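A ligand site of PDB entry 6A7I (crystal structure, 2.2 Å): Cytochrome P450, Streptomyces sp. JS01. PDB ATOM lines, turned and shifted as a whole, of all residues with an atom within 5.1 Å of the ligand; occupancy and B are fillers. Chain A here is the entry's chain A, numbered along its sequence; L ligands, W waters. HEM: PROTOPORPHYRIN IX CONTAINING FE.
N of Cys 352 lies within hydrogen-bond range of O of Phe 345 (2.8 Å). NH1 of Arg 100 lies within hydrogen-bond range of O of Val 351 (2.9 Å). NZ of Lys 59 sits at hydrogen-bond distance from O of Leu 89 (3.0 Å). The guanidinium group (NH1) of Arg 100 is in hydrogen-bond range of the backbone carbonyl oxygen (O) of Pro 349. A ring nitrogen (ND1) of His 350 lies close to the backbone carbonyl oxygen (O) of Met 88 (3.5 Å). SG of Cys 352 lies close to N of Gly 354 (3.3 Å). The backbone carbonyl oxygen (O) of Ala 240 sits at hydrogen-bond distance from the side-chain hydroxyl (OG1) of Thr 245, at 3.1 Å.
The guanidinium group (NH1) of Arg 100 is in salt-bridge range of an oxygen (O1D) of the ligand (2.7 Å). A ring nitrogen (NE2) of His 96 is in hydrogen-bond range of an oxygen (O1D) of the ligand (2.8 Å). The guanidinium group (NH2) of Arg 293 lies within salt-bridge range of an oxygen (O2A) of the ligand. An oxygen (O2D) of the ligand is in hydrogen-bond range of a ring nitrogen (ND1) of His 350 (2.7 Å). SG of Cys 352 binds FE of the ligand (2.3 Å). The side-chain amino group of Lys 59 is in salt-bridge range of an oxygen (O1A) of the ligand (2.9 Å).
The backbone carbonyl oxygen (O) of Met 88 sits close to an oxygen (O2D) of the ligand. Leu 89 touches the ligand (CA to O2D, 3.4 Å). Leu 107 touches the ligand. CD1 of Ile 154 touches CAC of the ligand (3.9 Å). Leu 236 touches the ligand (CD2 to CMD, 3.7 Å). Ile 237 touches the ligand (CG2 to CBC, 3.4 Å). CB of Ala 240 touches C1C of the ligand, 3.7 Å away. Thr 244 touches the ligand. Thr 245 touches the ligand. Leu 248 touches the ligand (CD2 to CBB, 3.98 Å). CG1 of Val 290 touches O1A of the ligand (3.3 Å). Phe 316 touches the ligand (CE2 to CMA, 3.3 Å). Ala 344 touches the ligand (O to CMA, 3.4 Å). C of Phe 345 touches CMA of the ligand, at 3.6 Å. Gly 346 touches the ligand (N to CMA, 3.7 Å). O of Pro 349 touches O1D of the ligand, at 3.9 Å. CD of Pro 353 touches C2D of the ligand, 3.6 Å away. Gly 354 touches the ligand. Ser 358 touches the ligand. Within 4 Å of the ligand: Lys 59, Met 88, Leu 89, His 96, Arg 100, Leu 107, Ile 154, Leu 236, Ile 237, Ala 240, Thr 244, Thr 245, Leu 248, Val 290, Arg 293, Phe 316, Ala 344, Phe 345, Gly 346, Pro 349, His 350, Cys 352, Pro 353, Gly 354 and Ser 358. The nearest printed residue that does not touch the ligand is Pro 286 (4.2 Å).
Water W2 lies within hydrogen-bond range of an oxygen (O1A) of the ligand (2.6 Å) and the backbone carbonyl oxygen (O) of Leu 291 (2.8 Å).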
ATOM      1  N   LEU A  52      -9.367  12.428 -29.864  1.00  0.00           N
ATOM      2  CA  LEU A  52      -8.927  11.148 -30.341  1.00  0.00           C
ATOM      3  C   LEU A  52      -9.965  10.539 -31.275  1.00  0.00           C
ATOM      4  O   LEU A  52      -9.645   9.604 -31.989  1.00  0.00           O
ATOM      5  CB  LEU A  52      -8.709  10.229 -29.146  1.00  0.00           C
ATOM      6  CG  LEU A  52      -7.427  10.406 -28.375  1.00  0.00           C
ATOM      7  CD1 LEU A  52      -7.450   9.633 -27.071  1.00  0.00           C
ATOM      8  CD2 LEU A  52      -6.249   9.926 -29.240  1.00  0.00           C
ATOM      9  N   LYS A  59      -2.693  11.348 -38.289  1.00  0.00           N
ATOM     10  CA  LYS A  59      -1.297  10.893 -38.143  1.00  0.00           C
ATOM     11  C   LYS A  59      -0.395  11.172 -39.316  1.00  0.00           C
ATOM     12  O   LYS A  59       0.737  10.733 -39.323  1.00  0.00           O
ATOM     13  CB  LYS A  59      -1.279   9.428 -37.935  1.00  0.00           C
ATOM     14  CG  LYS A  59      -2.037   8.988 -36.713  1.00  0.00           C
ATOM     15  CD  LYS A  59      -1.258   9.272 -35.468  1.00  0.00           C
ATOM     16  CE  LYS A  59      -1.681   8.335 -34.346  1.00  0.00           C
ATOM     17  NZ  LYS A  59      -0.617   7.449 -33.860  1.00  0.00           N
ATOM     18  N   MET A  88      -0.374   0.507 -39.296  1.00  0.00           N
ATOM     19  CA  MET A  88      -1.653   0.933 -38.749  1.00  0.00           C
ATOM     20  C   MET A  88      -1.557   2.155 -37.855  1.00  0.00           C
ATOM     21  O   MET A  88      -2.487   2.932 -37.783  1.00  0.00           O
ATOM     22  CB  MET A  88      -2.288  -0.224 -37.924  1.00  0.00           C
ATOM     23  CG  MET A  88      -1.684  -0.479 -36.536  1.00  0.00           C
ATOM     24  SD  MET A  88      -2.620  -1.841 -35.799  1.00  0.00           S
ATOM     25  CE  MET A  88      -1.578  -3.235 -36.260  1.00  0.00           C
ATOM     26  N   LEU A  89      -0.409   2.329 -37.200  1.00  0.00           N
ATOM     27  CA  LEU A  89      -0.236   3.429 -36.286  1.00  0.00           C
ATOM     28  C   LEU A  89      -0.163   4.776 -36.987  1.00  0.00           C
ATOM     29  O   LEU A  89      -0.456   5.801 -36.363  1.00  0.00           O
ATOM     30  CB  LEU A  89       1.049   3.237 -35.487  1.00  0.00           C
ATOM     31  CG  LEU A  89       1.365   4.216 -34.377  1.00  0.00           C
ATOM     32  CD1 LEU A  89       0.285   4.168 -33.293  1.00  0.00           C
ATOM     33  CD2 LEU A  89       2.761   3.950 -33.809  1.00  0.00           C
ATOM     34  N   HIS A  96      -6.275   2.420 -42.519  1.00  0.00           N
ATOM     35  CA  HIS A  96      -6.081   2.001 -41.120  1.00  0.00           C
ATOM     36  C   HIS A  96      -6.819   0.708 -40.863  1.00  0.00           C
ATOM     37  O   HIS A  96      -6.257  -0.210 -40.241  1.00  0.00           O
ATOM     38  CB  HIS A  96      -6.536   3.099 -40.147  1.00  0.00           C
ATOM     39  CG  HIS A  96      -6.511   2.680 -38.723  1.00  0.00           C
ATOM     40  ND1 HIS A  96      -7.652   2.415 -38.025  1.00  0.00           N
ATOM     41  CD2 HIS A  96      -5.482   2.385 -37.902  1.00  0.00           C
ATOM     42  CE1 HIS A  96      -7.342   2.003 -36.814  1.00  0.00           C
ATOM     43  NE2 HIS A  96      -6.024   2.012 -36.695  1.00  0.00           N
ATOM     44  N   ARG A 100      -4.962  -2.817 -39.749  1.00  0.00           N
ATOM     45  CA  ARG A 100      -5.249  -3.240 -38.325  1.00  0.00           C
ATOM     46  C   ARG A 100      -5.957  -4.607 -38.213  1.00  0.00           C
ATOM     47  O   ARG A 100      -5.744  -5.343 -37.237  1.00  0.00           O
ATOM     48  CB  ARG A 100      -6.144  -2.180 -37.647  1.00  0.00           C
ATOM     49  CG  ARG A 100      -6.393  -2.408 -36.166  1.00  0.00           C
ATOM     50  CD  ARG A 100      -7.214  -1.273 -35.624  1.00  0.00           C
ATOM     51  NE  ARG A 100      -7.793  -1.645 -34.332  1.00  0.00           N
ATOM     52  CZ  ARG A 100      -7.378  -1.235 -33.150  1.00  0.00           C
ATOM     53  NH1 ARG A 100      -6.358  -0.390 -33.022  1.00  0.00           N
ATOM     54  NH2 ARG A 100      -8.063  -1.591 -32.081  1.00  0.00           N
ATOM     55  N   VAL A 103      -4.308  -8.095 -36.994  1.00  0.00           N
ATOM     56  CA  VAL A 103      -3.706  -8.035 -35.652  1.00  0.00           C
ATOM     57  C   VAL A 103      -4.768  -7.929 -34.645  1.00  0.00           C
ATOM     58  O   VAL A 103      -4.726  -8.647 -33.647  1.00  0.00           O
ATOM     59  CB  VAL A 103      -2.684  -6.879 -35.504  1.00  0.00           C
ATOM     60  CG1 VAL A 103      -2.316  -6.634 -34.020  1.00  0.00           C
ATOM     61  CG2 VAL A 103      -1.435  -7.147 -36.328  1.00  0.00           C
ATOM     62  N   LEU A 107      -6.120 -10.866 -31.343  1.00  0.00           N
ATOM     63  CA  LEU A 107      -5.893 -10.429 -29.950  1.00  0.00           C
ATOM     64  C   LEU A 107      -7.180 -10.076 -29.225  1.00  0.00           C
ATOM     65  O   LEU A 107      -7.155  -9.368 -28.216  1.00  0.00           O
ATOM     66  CB  LEU A 107      -4.954  -9.208 -29.954  1.00  0.00           C
ATOM     67  CG  LEU A 107      -3.512  -9.391 -30.439  1.00  0.00           C
ATOM     68  CD1 LEU A 107      -2.778  -8.034 -30.593  1.00  0.00           C
ATOM     69  CD2 LEU A 107      -2.795 -10.312 -29.467  1.00  0.00           C
ATOM     70  N   ILE A 154       5.486 -11.819 -25.422  1.00  0.00           N
ATOM     71  CA  ILE A 154       5.317 -11.175 -26.701  1.00  0.00           C
ATOM     72  C   ILE A 154       6.184 -11.817 -27.823  1.00  0.00           C
ATOM     73  O   ILE A 154       5.734 -11.906 -28.988  1.00  0.00           O
ATOM     74  CB  ILE A 154       5.504  -9.636 -26.611  1.00  0.00           C
ATOM     75  CG1 ILE A 154       4.684  -8.924 -27.689  1.00  0.00           C
ATOM     76  CG2 ILE A 154       6.927  -9.206 -26.819  1.00  0.00           C
ATOM     77  CD1 ILE A 154       3.271  -8.759 -27.227  1.00  0.00           C
ATOM     78  N   LEU A 157       4.369 -14.939 -28.861  1.00  0.00           N
ATOM     79  CA  LEU A 157       3.210 -14.618 -29.703  1.00  0.00           C
ATOM     80  C   LEU A 157       3.622 -14.339 -31.169  1.00  0.00           C
ATOM     81  O   LEU A 157       2.939 -14.764 -32.064  1.00  0.00           O
ATOM     82  CB  LEU A 157       2.480 -13.401 -29.146  1.00  0.00           C
ATOM     83  CG  LEU A 157       1.418 -12.819 -30.082  1.00  0.00           C
ATOM     84  CD1 LEU A 157       0.172 -13.707 -29.988  1.00  0.00           C
ATOM     85  CD2 LEU A 157       1.133 -11.367 -29.740  1.00  0.00           C
ATOM     86  N   LEU A 236       6.587  -2.306 -33.975  1.00  0.00           N
ATOM     87  CA  LEU A 236       5.587  -1.682 -33.103  1.00  0.00           C
ATOM     88  C   LEU A 236       5.080  -2.672 -32.004  1.00  0.00           C
ATOM     89  O   LEU A 236       5.095  -2.353 -30.829  1.00  0.00           O
ATOM     90  CB  LEU A 236       4.461  -1.216 -34.005  1.00  0.00           C
ATOM     91  CG  LEU A 236       3.225  -0.661 -33.369  1.00  0.00           C
ATOM     92  CD1 LEU A 236       3.559   0.664 -32.688  1.00  0.00           C
ATOM     93  CD2 LEU A 236       2.214  -0.518 -34.501  1.00  0.00           C
ATOM     94  N   ILE A 237       4.802  -3.923 -32.375  1.00  0.00           N
ATOM     95  CA  ILE A 237       4.308  -4.899 -31.406  1.00  0.00           C
ATOM     96  C   ILE A 237       5.370  -5.260 -30.419  1.00  0.00           C
ATOM     97  O   ILE A 237       5.113  -5.302 -29.191  1.00  0.00           O
ATOM     98  CB  ILE A 237       3.695  -6.128 -32.048  1.00  0.00           C
ATOM     99  CG1 ILE A 237       2.406  -5.753 -32.770  1.00  0.00           C
ATOM    100  CG2 ILE A 237       3.411  -7.258 -30.996  1.00  0.00           C
ATOM    101  CD1 ILE A 237       1.919  -6.825 -33.712  1.00  0.00           C
ATOM    102  N   ALA A 240       6.178  -2.707 -27.365  1.00  0.00           N
ATOM    103  CA  ALA A 240       5.379  -3.015 -26.136  1.00  0.00           C
ATOM    104  C   ALA A 240       6.053  -3.967 -25.063  1.00  0.00           C
ATOM    105  O   ALA A 240       6.094  -3.694 -23.846  1.00  0.00           O
ATOM    106  CB  ALA A 240       4.041  -3.585 -26.557  1.00  0.00           C
ATOM    107  N   THR A 244       5.695  -1.083 -22.217  1.00  0.00           N
ATOM    108  CA  THR A 244       4.550  -0.688 -21.447  1.00  0.00           C
ATOM    109  C   THR A 244       4.118  -1.772 -20.484  1.00  0.00           C
ATOM    110  O   THR A 244       3.707  -1.489 -19.341  1.00  0.00           O
ATOM    111  CB  THR A 244       3.384  -0.295 -22.363  1.00  0.00           C
ATOM    112  OG1 THR A 244       3.236  -1.266 -23.379  1.00  0.00           O
ATOM    113  CG2 THR A 244       3.668   0.977 -23.052  1.00  0.00           C
ATOM    114  N   THR A 245       4.197  -3.019 -20.927  1.00  0.00           N
ATOM    115  CA  THR A 245       3.775  -4.156 -20.074  1.00  0.00           C
ATOM    116  C   THR A 245       4.689  -4.384 -18.832  1.00  0.00           C
ATOM    117  O   THR A 245       4.193  -4.639 -17.723  1.00  0.00           O
ATOM    118  CB  THR A 245       3.687  -5.450 -20.894  1.00  0.00           C
ATOM    119  OG1 THR A 245       4.936  -5.616 -21.640  1.00  0.00           O
ATOM    120  CG2 THR A 245       2.509  -5.355 -21.868  1.00  0.00           C
ATOM    121  N   LEU A 248       3.664  -1.555 -16.421  1.00  0.00           N
ATOM    122  CA  LEU A 248       2.464  -1.850 -15.655  1.00  0.00           C
ATOM    123  C   LEU A 248       2.762  -2.792 -14.433  1.00  0.00           C
ATOM    124  O   LEU A 248       2.315  -2.515 -13.324  1.00  0.00           O
ATOM    125  CB  LEU A 248       1.433  -2.433 -16.563  1.00  0.00           C
ATOM    126  CG  LEU A 248       0.201  -2.997 -15.940  1.00  0.00           C
ATOM    127  CD1 LEU A 248      -0.548  -1.860 -15.266  1.00  0.00           C
ATOM    128  CD2 LEU A 248      -0.569  -3.668 -17.065  1.00  0.00           C
ATOM    129  N   LEU A 281      -3.456   1.345 -14.202  1.00  0.00           N
ATOM    130  CA  LEU A 281      -3.537   1.892 -15.507  1.00  0.00           C
ATOM    131  C   LEU A 281      -4.099   3.318 -15.465  1.00  0.00           C
ATOM    132  O   LEU A 281      -3.615   4.172 -16.181  1.00  0.00           O
ATOM    133  CB  LEU A 281      -4.363   0.987 -16.424  1.00  0.00           C
ATOM    134  CG  LEU A 281      -3.700  -0.311 -16.848  1.00  0.00           C
ATOM    135  CD1 LEU A 281      -4.713  -1.319 -17.373  1.00  0.00           C
ATOM    136  CD2 LEU A 281      -2.623  -0.084 -17.847  1.00  0.00           C
ATOM    137  N   PRO A 286       1.364   3.473 -17.837  1.00  0.00           N
ATOM    138  CA  PRO A 286       2.668   3.211 -18.434  1.00  0.00           C
ATOM    139  C   PRO A 286       3.135   4.222 -19.484  1.00  0.00           C
ATOM    140  O   PRO A 286       4.262   4.502 -19.512  1.00  0.00           O
ATOM    141  CB  PRO A 286       2.530   1.838 -19.065  1.00  0.00           C
ATOM    142  CG  PRO A 286       1.522   1.143 -18.211  1.00  0.00           C
ATOM    143  CD  PRO A 286       0.586   2.235 -17.740  1.00  0.00           C
ATOM    144  N   THR A 287       2.239   4.785 -20.261  1.00  0.00           N
ATOM    145  CA  THR A 287       2.560   5.752 -21.278  1.00  0.00           C
ATOM    146  C   THR A 287       2.119   7.136 -20.858  1.00  0.00           C
ATOM    147  O   THR A 287       0.910   7.442 -20.815  1.00  0.00           O
ATOM    148  CB  THR A 287       1.832   5.365 -22.583  1.00  0.00           C
ATOM    149  OG1 THR A 287       2.292   4.080 -22.962  1.00  0.00           O
ATOM    150  CG2 THR A 287       2.188   6.336 -23.726  1.00  0.00           C
ATOM    151  N   VAL A 290       1.369  10.238 -25.537  1.00  0.00           N
ATOM    152  CA  VAL A 290       1.188   9.534 -26.794  1.00  0.00           C
ATOM    153  C   VAL A 290       1.552  10.520 -27.918  1.00  0.00           C
ATOM    154  O   VAL A 290       0.920  11.550 -28.052  1.00  0.00           O
ATOM    155  CB  VAL A 290      -0.263   9.103 -26.983  1.00  0.00           C
ATOM    156  CG1 VAL A 290      -0.451   8.451 -28.337  1.00  0.00           C
ATOM    157  CG2 VAL A 290      -0.701   8.178 -25.854  1.00  0.00           C
ATOM    158  N   LEU A 291       2.574  10.178 -28.685  1.00  0.00           N
ATOM    159  CA  LEU A 291       2.988  10.921 -29.865  1.00  0.00           C
ATOM    160  C   LEU A 291       2.505  10.173 -31.122  1.00  0.00           C
ATOM    161  O   LEU A 291       2.564   8.939 -31.146  1.00  0.00           O
ATOM    162  CB  LEU A 291       4.527  10.995 -29.934  1.00  0.00           C
ATOM    163  CG  LEU A 291       5.160  12.161 -29.236  1.00  0.00           C
ATOM    164  CD1 LEU A 291       4.823  12.158 -27.741  1.00  0.00           C
ATOM    165  CD2 LEU A 291       6.652  11.991 -29.434  1.00  0.00           C
ATOM    166  N   ARG A 293      -0.061  13.506 -33.174  1.00  0.00           N
ATOM    167  CA  ARG A 293      -1.090  13.802 -34.131  1.00  0.00           C
ATOM    168  C   ARG A 293      -0.961  15.222 -34.682  1.00  0.00           C
ATOM    169  O   ARG A 293      -0.340  16.058 -34.072  1.00  0.00           O
ATOM    170  CB  ARG A 293      -2.413  13.676 -33.412  1.00  0.00           C
ATOM    171  CG  ARG A 293      -2.812  12.204 -33.187  1.00  0.00           C
ATOM    172  CD  ARG A 293      -3.843  12.078 -32.046  1.00  0.00           C
ATOM    173  NE  ARG A 293      -4.415  10.740 -32.145  1.00  0.00           N
ATOM    174  CZ  ARG A 293      -3.812   9.614 -31.731  1.00  0.00           C
ATOM    175  NH1 ARG A 293      -2.661   9.626 -31.028  1.00  0.00           N
ATOM    176  NH2 ARG A 293      -4.407   8.474 -31.972  1.00  0.00           N
ATOM    177  N   PHE A 316      -1.485  11.289 -21.142  1.00  0.00           N
ATOM    178  CA  PHE A 316      -2.207  10.317 -20.347  1.00  0.00           C
ATOM    179  C   PHE A 316      -1.906  10.264 -18.894  1.00  0.00           C
ATOM    180  O   PHE A 316      -2.823   9.984 -18.120  1.00  0.00           O
ATOM    181  CB  PHE A 316      -1.916   8.918 -20.786  1.00  0.00           C
ATOM    182  CG  PHE A 316      -2.568   8.532 -22.005  1.00  0.00           C
ATOM    183  CD1 PHE A 316      -3.818   8.999 -22.316  1.00  0.00           C
ATOM    184  CD2 PHE A 316      -2.048   7.443 -22.682  1.00  0.00           C
ATOM    185  CE1 PHE A 316      -4.460   8.555 -23.396  1.00  0.00           C
ATOM    186  CE2 PHE A 316      -2.674   6.960 -23.750  1.00  0.00           C
ATOM    187  CZ  PHE A 316      -3.876   7.540 -24.151  1.00  0.00           C
ATOM    188  N   ALA A 344      -5.928   4.631 -20.654  1.00  0.00           N
ATOM    189  CA  ALA A 344      -4.530   4.225 -20.687  1.00  0.00           C
ATOM    190  C   ALA A 344      -4.141   3.584 -22.000  1.00  0.00           C
ATOM    191  O   ALA A 344      -2.971   3.654 -22.441  1.00  0.00           O
ATOM    192  CB  ALA A 344      -4.284   3.209 -19.581  1.00  0.00           C
ATOM    193  N   PHE A 345      -5.134   2.954 -22.628  1.00  0.00           N
ATOM    194  CA  PHE A 345      -4.947   2.266 -23.905  1.00  0.00           C
ATOM    195  C   PHE A 345      -5.375   3.093 -25.111  1.00  0.00           C
ATOM    196  O   PHE A 345      -5.415   2.604 -26.228  1.00  0.00           O
ATOM    197  CB  PHE A 345      -5.734   0.966 -23.887  1.00  0.00           C
ATOM    198  CG  PHE A 345      -5.212  -0.047 -22.927  1.00  0.00           C
ATOM    199  CD1 PHE A 345      -4.012  -0.662 -23.114  1.00  0.00           C
ATOM    200  CD2 PHE A 345      -5.988  -0.451 -21.877  1.00  0.00           C
ATOM    201  CE1 PHE A 345      -3.538  -1.632 -22.206  1.00  0.00           C
ATOM    202  CE2 PHE A 345      -5.543  -1.442 -20.989  1.00  0.00           C
ATOM    203  CZ  PHE A 345      -4.336  -2.025 -21.160  1.00  0.00           C
ATOM    204  N   GLY A 346      -5.722   4.351 -24.904  1.00  0.00           N
ATOM    205  CA  GLY A 346      -6.075   5.209 -26.018  1.00  0.00           C
ATOM    206  C   GLY A 346      -7.555   5.232 -26.096  1.00  0.00           C
ATOM    207  O   GLY A 346      -8.233   4.871 -25.167  1.00  0.00           O
ATOM    208  N   PRO A 349     -10.222   5.176 -33.067  1.00  0.00           N
ATOM    209  CA  PRO A 349      -9.840   4.079 -33.943  1.00  0.00           C
ATOM    210  C   PRO A 349      -8.449   3.421 -33.644  1.00  0.00           C
ATOM    211  O   PRO A 349      -8.253   2.265 -33.955  1.00  0.00           O
ATOM    212  CB  PRO A 349      -9.753   4.779 -35.303  1.00  0.00           C
ATOM    213  CG  PRO A 349     -10.656   5.945 -35.205  1.00  0.00           C
ATOM    214  CD  PRO A 349     -10.422   6.431 -33.797  1.00  0.00           C
ATOM    215  N   HIS A 350      -7.504   4.144 -33.041  1.00  0.00           N
ATOM    216  CA  HIS A 350      -6.191   3.600 -32.777  1.00  0.00           C
ATOM    217  C   HIS A 350      -6.116   2.987 -31.381  1.00  0.00           C
ATOM    218  O   HIS A 350      -5.031   2.632 -30.997  1.00  0.00           O
ATOM    219  CB  HIS A 350      -5.124   4.647 -32.931  1.00  0.00           C
ATOM    220  CG  HIS A 350      -4.973   5.137 -34.318  1.00  0.00           C
ATOM    221  ND1 HIS A 350      -4.062   4.596 -35.196  1.00  0.00           N
ATOM    222  CD2 HIS A 350      -5.598   6.132 -34.996  1.00  0.00           C
ATOM    223  CE1 HIS A 350      -4.124   5.250 -36.342  1.00  0.00           C
ATOM    224  NE2 HIS A 350      -5.059   6.167 -36.262  1.00  0.00           N
ATOM    225  N   VAL A 351      -7.240   2.798 -30.690  1.00  0.00           N
ATOM    226  CA  VAL A 351      -7.247   2.205 -29.346  1.00  0.00           C
ATOM    227  C   VAL A 351      -6.459   0.898 -29.306  1.00  0.00           C
ATOM    228  O   VAL A 351      -6.593   0.063 -30.216  1.00  0.00           O
ATOM    229  CB  VAL A 351      -8.648   2.045 -28.776  1.00  0.00           C
ATOM    230  CG1 VAL A 351      -9.483   0.911 -29.508  1.00  0.00           C
ATOM    231  CG2 VAL A 351      -8.598   1.757 -27.295  1.00  0.00           C
ATOM    232  N   CYS A 352      -5.629   0.725 -28.256  1.00  0.00           N
ATOM    233  CA  CYS A 352      -4.703  -0.432 -28.192  1.00  0.00           C
ATOM    234  C   CYS A 352      -5.418  -1.756 -28.557  1.00  0.00           C
ATOM    235  O   CYS A 352      -6.345  -2.121 -27.908  1.00  0.00           O
ATOM    236  CB  CYS A 352      -4.156  -0.665 -26.787  1.00  0.00           C
ATOM    237  SG  CYS A 352      -2.736  -1.843 -26.761  1.00  0.00           S
ATOM    238  N   PRO A 353      -4.914  -2.484 -29.516  1.00  0.00           N
ATOM    239  CA  PRO A 353      -5.510  -3.809 -29.788  1.00  0.00           C
ATOM    240  C   PRO A 353      -4.926  -4.898 -28.908  1.00  0.00           C
ATOM    241  O   PRO A 353      -5.477  -5.980 -28.813  1.00  0.00           O
ATOM    242  CB  PRO A 353      -5.140  -4.055 -31.251  1.00  0.00           C
ATOM    243  CG  PRO A 353      -3.838  -3.356 -31.395  1.00  0.00           C
ATOM    244  CD  PRO A 353      -4.013  -2.078 -30.597  1.00  0.00           C
ATOM    245  N   GLY A 354      -3.811  -4.622 -28.264  1.00  0.00           N
ATOM    246  CA  GLY A 354      -3.196  -5.553 -27.334  1.00  0.00           C
ATOM    247  C   GLY A 354      -3.667  -5.465 -25.893  1.00  0.00           C
ATOM    248  O   GLY A 354      -3.075  -6.084 -25.020  1.00  0.00           O
ATOM    249  N   LEU A 357      -4.433  -8.722 -24.064  1.00  0.00           N
ATOM    250  CA  LEU A 357      -3.180  -9.475 -23.772  1.00  0.00           C
ATOM    251  C   LEU A 357      -2.437  -8.919 -22.571  1.00  0.00           C
ATOM    252  O   LEU A 357      -2.015  -9.684 -21.685  1.00  0.00           O
ATOM    253  CB  LEU A 357      -2.259  -9.488 -24.957  1.00  0.00           C
ATOM    254  CG  LEU A 357      -0.933 -10.231 -24.756  1.00  0.00           C
ATOM    255  CD1 LEU A 357      -1.166 -11.637 -24.291  1.00  0.00           C
ATOM    256  CD2 LEU A 357      -0.152 -10.220 -26.031  1.00  0.00           C
ATOM    257  N   SER A 358      -2.311  -7.592 -22.477  1.00  0.00           N
ATOM    258  CA  SER A 358      -1.568  -7.014 -21.389  1.00  0.00           C
ATOM    259  C   SER A 358      -2.289  -7.223 -20.089  1.00  0.00           C
ATOM    260  O   SER A 358      -1.631  -7.503 -19.038  1.00  0.00           O
ATOM    261  CB  SER A 358      -1.241  -5.531 -21.637  1.00  0.00           C
ATOM    262  OG  SER A 358      -2.424  -4.782 -21.549  1.00  0.00           O
ATOM    263  N   GLU A 361      -1.600 -11.092 -19.082  1.00  0.00           N
ATOM    264  CA  GLU A 361      -0.219 -11.200 -18.553  1.00  0.00           C
ATOM    265  C   GLU A 361      -0.039 -10.654 -17.154  1.00  0.00           C
ATOM    266  O   GLU A 361       0.580 -11.275 -16.307  1.00  0.00           O
ATOM    267  CB  GLU A 361       0.730 -10.379 -19.345  1.00  0.00           C
ATOM    268  CG  GLU A 361       1.165 -10.842 -20.690  1.00  0.00           C
ATOM    269  CD  GLU A 361       2.334  -9.975 -21.189  1.00  0.00           C
ATOM    270  OE1 GLU A 361       3.365  -9.963 -20.476  1.00  0.00           O
ATOM    271  OE2 GLU A 361       2.211  -9.267 -22.244  1.00  0.00           O
HETATM  272  CHA HEM L   1      -1.567   1.413 -29.659  1.00  0.00           C
HETATM  273  CHB HEM L   1      -0.955   1.675 -24.867  1.00  0.00           C
HETATM  274  CHC HEM L   1       0.248  -3.054 -24.857  1.00  0.00           C
HETATM  275  CHD HEM L   1       0.017  -3.131 -29.669  1.00  0.00           C
HETATM  276  C1A HEM L   1      -1.585   1.853 -28.336  1.00  0.00           C
HETATM  277  C2A HEM L   1      -2.015   3.154 -27.928  1.00  0.00           C
HETATM  278  C3A HEM L   1      -1.818   3.222 -26.595  1.00  0.00           C
HETATM  279  C4A HEM L   1      -1.233   2.007 -26.182  1.00  0.00           C
HETATM  280  CMA HEM L   1      -2.094   4.382 -25.671  1.00  0.00           C
HETATM  281  CAA HEM L   1      -2.600   4.224 -28.830  1.00  0.00           C
HETATM  282  CBA HEM L   1      -1.579   4.994 -29.644  1.00  0.00           C
HETATM  283  CGA HEM L   1      -2.195   6.204 -30.376  1.00  0.00           C
HETATM  284  O1A HEM L   1      -1.422   6.912 -31.113  1.00  0.00           O
HETATM  285  O2A HEM L   1      -3.428   6.460 -30.301  1.00  0.00           O
HETATM  286  C1B HEM L   1      -0.556   0.380 -24.415  1.00  0.00           C
HETATM  287  C2B HEM L   1      -0.393  -0.001 -23.026  1.00  0.00           C
HETATM  288  C3B HEM L   1      -0.030  -1.319 -23.005  1.00  0.00           C
HETATM  289  C4B HEM L   1      -0.032  -1.754 -24.427  1.00  0.00           C
HETATM  290  CMB HEM L   1      -0.546   0.907 -21.872  1.00  0.00           C
HETATM  291  CAB HEM L   1       0.268  -2.222 -21.899  1.00  0.00           C
HETATM  292  CBB HEM L   1       0.008  -1.967 -20.612  1.00  0.00           C
HETATM  293  C1C HEM L   1       0.340  -3.527 -26.147  1.00  0.00           C
HETATM  294  C2C HEM L   1       0.519  -4.854 -26.515  1.00  0.00           C
HETATM  295  C3C HEM L   1       0.467  -4.915 -27.901  1.00  0.00           C
HETATM  296  C4C HEM L   1       0.207  -3.567 -28.358  1.00  0.00           C
HETATM  297  CMC HEM L   1       0.766  -6.030 -25.633  1.00  0.00           C
HETATM  298  CAC HEM L   1       0.609  -6.241 -28.551  1.00  0.00           C
HETATM  299  CBC HEM L   1       0.331  -6.460 -29.800  1.00  0.00           C
HETATM  300  C1D HEM L   1      -0.431  -1.866 -30.009  1.00  0.00           C
HETATM  301  C2D HEM L   1      -0.579  -1.514 -31.403  1.00  0.00           C
HETATM  302  C3D HEM L   1      -1.024  -0.271 -31.435  1.00  0.00           C
HETATM  303  C4D HEM L   1      -1.092   0.136 -30.023  1.00  0.00           C
HETATM  304  CMD HEM L   1      -0.307  -2.426 -32.591  1.00  0.00           C
HETATM  305  CAD HEM L   1      -1.355   0.549 -32.686  1.00  0.00           C
HETATM  306  CBD HEM L   1      -2.880   0.421 -32.933  1.00  0.00           C
HETATM  307  CGD HEM L   1      -3.459   1.320 -34.009  1.00  0.00           C
HETATM  308  O1D HEM L   1      -4.579   1.051 -34.489  1.00  0.00           O
HETATM  309  O2D HEM L   1      -2.846   2.328 -34.457  1.00  0.00           O
HETATM  310  NA  HEM L   1      -1.148   1.147 -27.248  1.00  0.00           N
HETATM  311  NB  HEM L   1      -0.353  -0.695 -25.185  1.00  0.00           N
HETATM  312  NC  HEM L   1       0.147  -2.765 -27.258  1.00  0.00           N
HETATM  313  ND  HEM L   1      -0.735  -0.859 -29.189  1.00  0.00           N
HETATM  314 FE   HEM L   1      -0.742  -0.857 -27.237  1.00  0.00          FE
HETATM  315  O   HOH W   1      -5.767   5.852 -29.343  1.00  0.00           O
HETATM  316  O   HOH W   2       1.120   6.583 -30.771  1.00  0.00           O
